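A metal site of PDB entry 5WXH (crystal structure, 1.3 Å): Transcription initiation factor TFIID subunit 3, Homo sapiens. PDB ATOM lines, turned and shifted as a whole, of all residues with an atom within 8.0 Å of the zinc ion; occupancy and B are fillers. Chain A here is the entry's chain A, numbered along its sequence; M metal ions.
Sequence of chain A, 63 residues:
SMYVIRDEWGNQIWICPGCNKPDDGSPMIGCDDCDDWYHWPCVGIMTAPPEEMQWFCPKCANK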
ATOM      1  N   ILE A  15      15.831 -14.877 -23.389  1.00  0.00           N
ATOM      2  CA  ILE A  15      16.673 -15.849 -22.696  1.00  0.00           C
ATOM      3  C   ILE A  15      16.359 -17.244 -23.213  1.00  0.00           C
ATOM      4  O   ILE A  15      15.182 -17.604 -23.355  1.00  0.00           O
ATOM      5  CB  ILE A  15      16.452 -15.761 -21.168  1.00  0.00           C
ATOM      6  CG1 ILE A  15      16.703 -14.326 -20.654  1.00  0.00           C
ATOM      7  CG2 ILE A  15      17.313 -16.773 -20.454  1.00  0.00           C
ATOM      8  CD1 ILE A  15      18.080 -13.800 -20.898  1.00  0.00           C
ATOM      9  N   CYS A  16      17.397 -18.015 -23.484  1.00  0.00           N
ATOM     10  CA  CYS A  16      17.237 -19.410 -23.907  1.00  0.00           C
ATOM     11  C   CYS A  16      16.855 -20.263 -22.706  1.00  0.00           C
ATOM     12  O   CYS A  16      17.586 -20.288 -21.713  1.00  0.00           O
ATOM     13  CB  CYS A  16      18.566 -19.896 -24.456  1.00  0.00           C
ATOM     14  SG  CYS A  16      18.634 -21.648 -24.876  1.00  0.00           S
ATOM     15  N   PRO A  17      15.720 -20.976 -22.751  1.00  0.00           N
ATOM     16  CA  PRO A  17      15.351 -21.818 -21.606  1.00  0.00           C
ATOM     17  C   PRO A  17      16.293 -22.990 -21.387  1.00  0.00           C
ATOM     18  O   PRO A  17      16.286 -23.570 -20.283  1.00  0.00           O
ATOM     19  CB  PRO A  17      13.933 -22.298 -21.963  1.00  0.00           C
ATOM     20  CG  PRO A  17      13.432 -21.281 -22.950  1.00  0.00           C
ATOM     21  CD  PRO A  17      14.633 -20.875 -23.736  1.00  0.00           C
ATOM     22  N   GLY A  18      17.117 -23.342 -22.374  1.00  0.00           N
ATOM     23  CA  GLY A  18      17.998 -24.486 -22.207  1.00  0.00           C
ATOM     24  C   GLY A  18      19.167 -24.169 -21.294  1.00  0.00           C
ATOM     25  O   GLY A  18      19.569 -25.004 -20.472  1.00  0.00           O
ATOM     26  N   CYS A  19      19.729 -22.964 -21.406  1.00  0.00           N
ATOM     27  CA  CYS A  19      20.924 -22.595 -20.672  1.00  0.00           C
ATOM     28  C   CYS A  19      20.754 -21.373 -19.784  1.00  0.00           C
ATOM     29  O   CYS A  19      21.682 -21.045 -19.036  1.00  0.00           O
ATOM     30  CB  CYS A  19      22.093 -22.359 -21.630  1.00  0.00           C
ATOM     31  SG  CYS A  19      21.846 -20.971 -22.755  1.00  0.00           S
ATOM     32  N   ASN A  20      19.611 -20.689 -19.837  1.00  0.00           N
ATOM     33  CA  ASN A  20      19.351 -19.486 -19.049  1.00  0.00           C
ATOM     34  C   ASN A  20      20.316 -18.341 -19.376  1.00  0.00           C
ATOM     35  O   ASN A  20      20.561 -17.479 -18.537  1.00  0.00           O
ATOM     36  CB  ASN A  20      19.306 -19.768 -17.551  1.00  0.00           C
ATOM     37  CG  ASN A  20      18.290 -20.822 -17.204  1.00  0.00           C
ATOM     38  OD1 ASN A  20      18.613 -21.848 -16.607  1.00  0.00           O
ATOM     39  ND2 ASN A  20      17.048 -20.586 -17.595  1.00  0.00           N
ATOM     40  N   LYS A  21      20.847 -18.326 -20.585  1.00  0.00           N
ATOM     41  CA  LYS A  21      21.669 -17.232 -21.036  1.00  0.00           C
ATOM     42  C   LYS A  21      20.972 -16.484 -22.161  1.00  0.00           C
ATOM     43  O   LYS A  21      20.173 -17.075 -22.906  1.00  0.00           O
ATOM     44  CB  LYS A  21      23.031 -17.714 -21.549  1.00  0.00           C
ATOM     45  CG  LYS A  21      23.889 -18.411 -20.513  1.00  0.00           C
ATOM     46  CD  LYS A  21      25.220 -18.838 -21.131  1.00  0.00           C
ATOM     47  CE  LYS A  21      26.108 -19.551 -20.131  1.00  0.00           C
ATOM     48  NZ  LYS A  21      27.436 -19.883 -20.719  1.00  0.00           N
ATOM     49  N   PRO A  22      21.268 -15.205 -22.347  1.00  0.00           N
ATOM     50  CA  PRO A  22      20.581 -14.429 -23.391  1.00  0.00           C
ATOM     51  C   PRO A  22      21.009 -14.823 -24.794  1.00  0.00           C
ATOM     52  O   PRO A  22      22.060 -15.428 -25.036  1.00  0.00           O
ATOM     53  CB  PRO A  22      20.996 -12.982 -23.108  1.00  0.00           C
ATOM     54  CG  PRO A  22      21.602 -12.986 -21.753  1.00  0.00           C
ATOM     55  CD  PRO A  22      22.131 -14.355 -21.509  1.00  0.00           C
ATOM     56  N   ASP A  23      20.149 -14.452 -25.729  1.00  0.00           N
ATOM     57  CA  ASP A  23      20.545 -14.272 -27.111  1.00  0.00           C
ATOM     58  C   ASP A  23      21.808 -13.419 -27.176  1.00  0.00           C
ATOM     59  O   ASP A  23      21.858 -12.329 -26.585  1.00  0.00           O
ATOM     60  CB  ASP A  23      19.379 -13.550 -27.797  1.00  0.00           C
ATOM     61  CG  ASP A  23      19.618 -13.241 -29.252  1.00  0.00           C
ATOM     62  OD1 ASP A  23      20.583 -13.749 -29.869  1.00  0.00           O
ATOM     63  OD2 ASP A  23      18.786 -12.491 -29.789  1.00  0.00           O
ATOM     64  N   SER A  26      24.315 -15.441 -31.726  1.00  0.00           N
ATOM     65  CA  SER A  26      24.515 -16.752 -32.311  1.00  0.00           C
ATOM     66  C   SER A  26      23.161 -17.347 -32.733  1.00  0.00           C
ATOM     67  O   SER A  26      22.110 -16.858 -32.324  1.00  0.00           O
ATOM     68  CB  SER A  26      25.220 -17.665 -31.305  1.00  0.00           C
ATOM     69  OG  SER A  26      24.438 -17.868 -30.158  1.00  0.00           O
ATOM     70  N   PRO A  27      23.164 -18.382 -33.577  1.00  0.00           N
ATOM     71  CA  PRO A  27      21.895 -18.869 -34.132  1.00  0.00           C
ATOM     72  C   PRO A  27      20.900 -19.329 -33.062  1.00  0.00           C
ATOM     73  O   PRO A  27      21.261 -20.052 -32.133  1.00  0.00           O
ATOM     74  CB  PRO A  27      22.331 -20.021 -35.035  1.00  0.00           C
ATOM     75  CG  PRO A  27      23.718 -19.650 -35.457  1.00  0.00           C
ATOM     76  CD  PRO A  27      24.323 -18.998 -34.244  1.00  0.00           C
ATOM     77  N   MET A  28      19.653 -18.891 -33.218  1.00  0.00           N
ATOM     78  CA  MET A  28      18.554 -19.317 -32.378  1.00  0.00           C
ATOM     79  C   MET A  28      17.419 -19.841 -33.241  1.00  0.00           C
ATOM     80  O   MET A  28      17.348 -19.579 -34.452  1.00  0.00           O
ATOM     81  CB  MET A  28      18.048 -18.175 -31.483  1.00  0.00           C
ATOM     82  CG  MET A  28      19.079 -17.621 -30.529  1.00  0.00           C
ATOM     83  SD  MET A  28      18.377 -16.501 -29.307  1.00  0.00           S
ATOM     84  CE  MET A  28      17.985 -17.643 -27.974  1.00  0.00           C
ATOM     85  N   TRP A  37      12.547 -18.918 -27.557  1.00  0.00           N
ATOM     86  CA  TRP A  37      13.693 -18.970 -28.466  1.00  0.00           C
ATOM     87  C   TRP A  37      14.858 -19.679 -27.780  1.00  0.00           C
ATOM     88  O   TRP A  37      15.181 -19.372 -26.626  1.00  0.00           O
ATOM     89  CB  TRP A  37      14.108 -17.562 -28.893  1.00  0.00           C
ATOM     90  CG  TRP A  37      13.171 -16.980 -29.911  1.00  0.00           C
ATOM     91  CD1 TRP A  37      11.995 -16.319 -29.679  1.00  0.00           C
ATOM     92  CD2 TRP A  37      13.316 -17.036 -31.343  1.00  0.00           C
ATOM     93  NE1 TRP A  37      11.410 -15.953 -30.871  1.00  0.00           N
ATOM     94  CE2 TRP A  37      12.208 -16.380 -31.902  1.00  0.00           C
ATOM     95  CE3 TRP A  37      14.294 -17.561 -32.188  1.00  0.00           C
ATOM     96  CZ2 TRP A  37      12.040 -16.242 -33.281  1.00  0.00           C
ATOM     97  CZ3 TRP A  37      14.123 -17.422 -33.553  1.00  0.00           C
ATOM     98  CH2 TRP A  37      13.017 -16.770 -34.076  1.00  0.00           C
ATOM     99  N   TYR A  38      15.483 -20.609 -28.494  1.00  0.00           N
ATOM    100  CA  TYR A  38      16.589 -21.410 -27.969  1.00  0.00           C
ATOM    101  C   TYR A  38      17.816 -21.237 -28.851  1.00  0.00           C
ATOM    102  O   TYR A  38      17.690 -21.163 -30.078  1.00  0.00           O
ATOM    103  CB  TYR A  38      16.226 -22.891 -27.976  1.00  0.00           C
ATOM    104  CG  TYR A  38      15.236 -23.345 -26.926  1.00  0.00           C
ATOM    105  CD1 TYR A  38      15.654 -24.096 -25.837  1.00  0.00           C
ATOM    106  CD2 TYR A  38      13.884 -23.044 -27.033  1.00  0.00           C
ATOM    107  CE1 TYR A  38      14.747 -24.539 -24.885  1.00  0.00           C
ATOM    108  CE2 TYR A  38      12.975 -23.479 -26.075  1.00  0.00           C
ATOM    109  CZ  TYR A  38      13.420 -24.224 -25.016  1.00  0.00           C
ATOM    110  OH  TYR A  38      12.522 -24.652 -24.064  1.00  0.00           O
ATOM    111  N   HIS A  39      19.002 -21.218 -28.243  1.00  0.00           N
ATOM    112  CA  HIS A  39      20.220 -21.366 -29.035  1.00  0.00           C
ATOM    113  C   HIS A  39      20.217 -22.722 -29.707  1.00  0.00           C
ATOM    114  O   HIS A  39      19.839 -23.732 -29.107  1.00  0.00           O
ATOM    115  CB  HIS A  39      21.465 -21.310 -28.153  1.00  0.00           C
ATOM    116  CG  HIS A  39      21.580 -20.091 -27.300  1.00  0.00           C
ATOM    117  ND1 HIS A  39      21.478 -20.144 -25.932  1.00  0.00           N
ATOM    118  CD2 HIS A  39      21.811 -18.789 -27.611  1.00  0.00           C
ATOM    119  CE1 HIS A  39      21.633 -18.936 -25.433  1.00  0.00           C
ATOM    120  NE2 HIS A  39      21.835 -18.090 -26.428  1.00  0.00           N
ATOM    121  N   TRP A  40      20.671 -22.764 -30.966  1.00  0.00           N
ATOM    122  CA  TRP A  40      20.724 -24.042 -31.682  1.00  0.00           C
ATOM    123  C   TRP A  40      21.390 -25.165 -30.897  1.00  0.00           C
ATOM    124  O   TRP A  40      20.789 -26.244 -30.788  1.00  0.00           O
ATOM    125  CB  TRP A  40      21.417 -23.917 -33.049  1.00  0.00           C
ATOM    126  CG  TRP A  40      20.643 -23.233 -34.136  1.00  0.00           C
ATOM    127  CD1 TRP A  40      19.501 -22.501 -34.025  1.00  0.00           C
ATOM    128  CD2 TRP A  40      20.989 -23.240 -35.517  1.00  0.00           C
ATOM    129  NE1 TRP A  40      19.105 -22.044 -35.265  1.00  0.00           N
ATOM    130  CE2 TRP A  40      20.013 -22.479 -36.191  1.00  0.00           C
ATOM    131  CE3 TRP A  40      22.036 -23.803 -36.250  1.00  0.00           C
ATOM    132  CZ2 TRP A  40      20.047 -22.274 -37.570  1.00  0.00           C
ATOM    133  CZ3 TRP A  40      22.069 -23.604 -37.622  1.00  0.00           C
ATOM    134  CH2 TRP A  40      21.093 -22.840 -38.252  1.00  0.00           C
ATOM    135  N   PRO A  41      22.610 -24.993 -30.348  1.00  0.00           N
ATOM    136  CA  PRO A  41      23.229 -26.140 -29.661  1.00  0.00           C
ATOM    137  C   PRO A  41      22.442 -26.615 -28.461  1.00  0.00           C
ATOM    138  O   PRO A  41      22.478 -27.804 -28.139  1.00  0.00           O
ATOM    139  CB  PRO A  41      24.618 -25.624 -29.276  1.00  0.00           C
ATOM    140  CG  PRO A  41      24.492 -24.161 -29.287  1.00  0.00           C
ATOM    141  CD  PRO A  41      23.502 -23.828 -30.360  1.00  0.00           C
ATOM    142  N   CYS A  42      21.718 -25.701 -27.806  1.00  0.00           N
ATOM    143  CA  CYS A  42      20.967 -26.069 -26.612  1.00  0.00           C
ATOM    144  C   CYS A  42      19.828 -27.036 -26.925  1.00  0.00           C
ATOM    145  O   CYS A  42      19.299 -27.668 -25.998  1.00  0.00           O
ATOM    146  CB  CYS A  42      20.470 -24.801 -25.927  1.00  0.00           C
ATOM    147  SG  CYS A  42      21.851 -23.774 -25.343  1.00  0.00           S
ATOM    148  N   VAL A  43      19.436 -27.177 -28.185  1.00  0.00           N
ATOM    149  CA  VAL A  43      18.376 -28.083 -28.593  1.00  0.00           C
ATOM    150  C   VAL A  43      18.840 -29.035 -29.677  1.00  0.00           C
ATOM    151  O   VAL A  43      18.024 -29.652 -30.380  1.00  0.00           O
ATOM    152  CB  VAL A  43      17.100 -27.334 -29.030  1.00  0.00           C
ATOM    153  CG1 VAL A  43      16.424 -26.717 -27.822  1.00  0.00           C
ATOM    154  CG2 VAL A  43      17.443 -26.272 -30.079  1.00  0.00           C
HETATM  155 ZN    ZN M   1      20.968 -21.790 -24.704  1.00  0.00          ZN
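The side-chain sulfur (SG) of Cys 16 lies close to the backbone NH (N) of Gly 18, 3.4 Å away.
O of Lys 21 is in hydrogen-bond range of N of Cys 16 (3.0 Å).
The backbone NH of Lys 21 sits close to the side-chain sulfur of Cys 19 (3.6 Å).
O of Pro 22 lies within hydrogen-bond range of NE2 of His 39, 3.0 Å away.
Four residues have an atom within 4 Å of the zinc ion: Cys 16, Cys 19, His 39 and Cys 42.
The nearest printed residue that does not touch the zinc ion is Gly 18 (4.5 Å).
The zinc ion is bound by a ring nitrogen (ND1) of His 39 (2.1 Å), the side-chain sulfur of Cys 42 (2.3 Å), the side-chain sulfur of Cys 19 (2.3 Å) and the side-chain sulfur of Cys 16 (2.3 Å).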
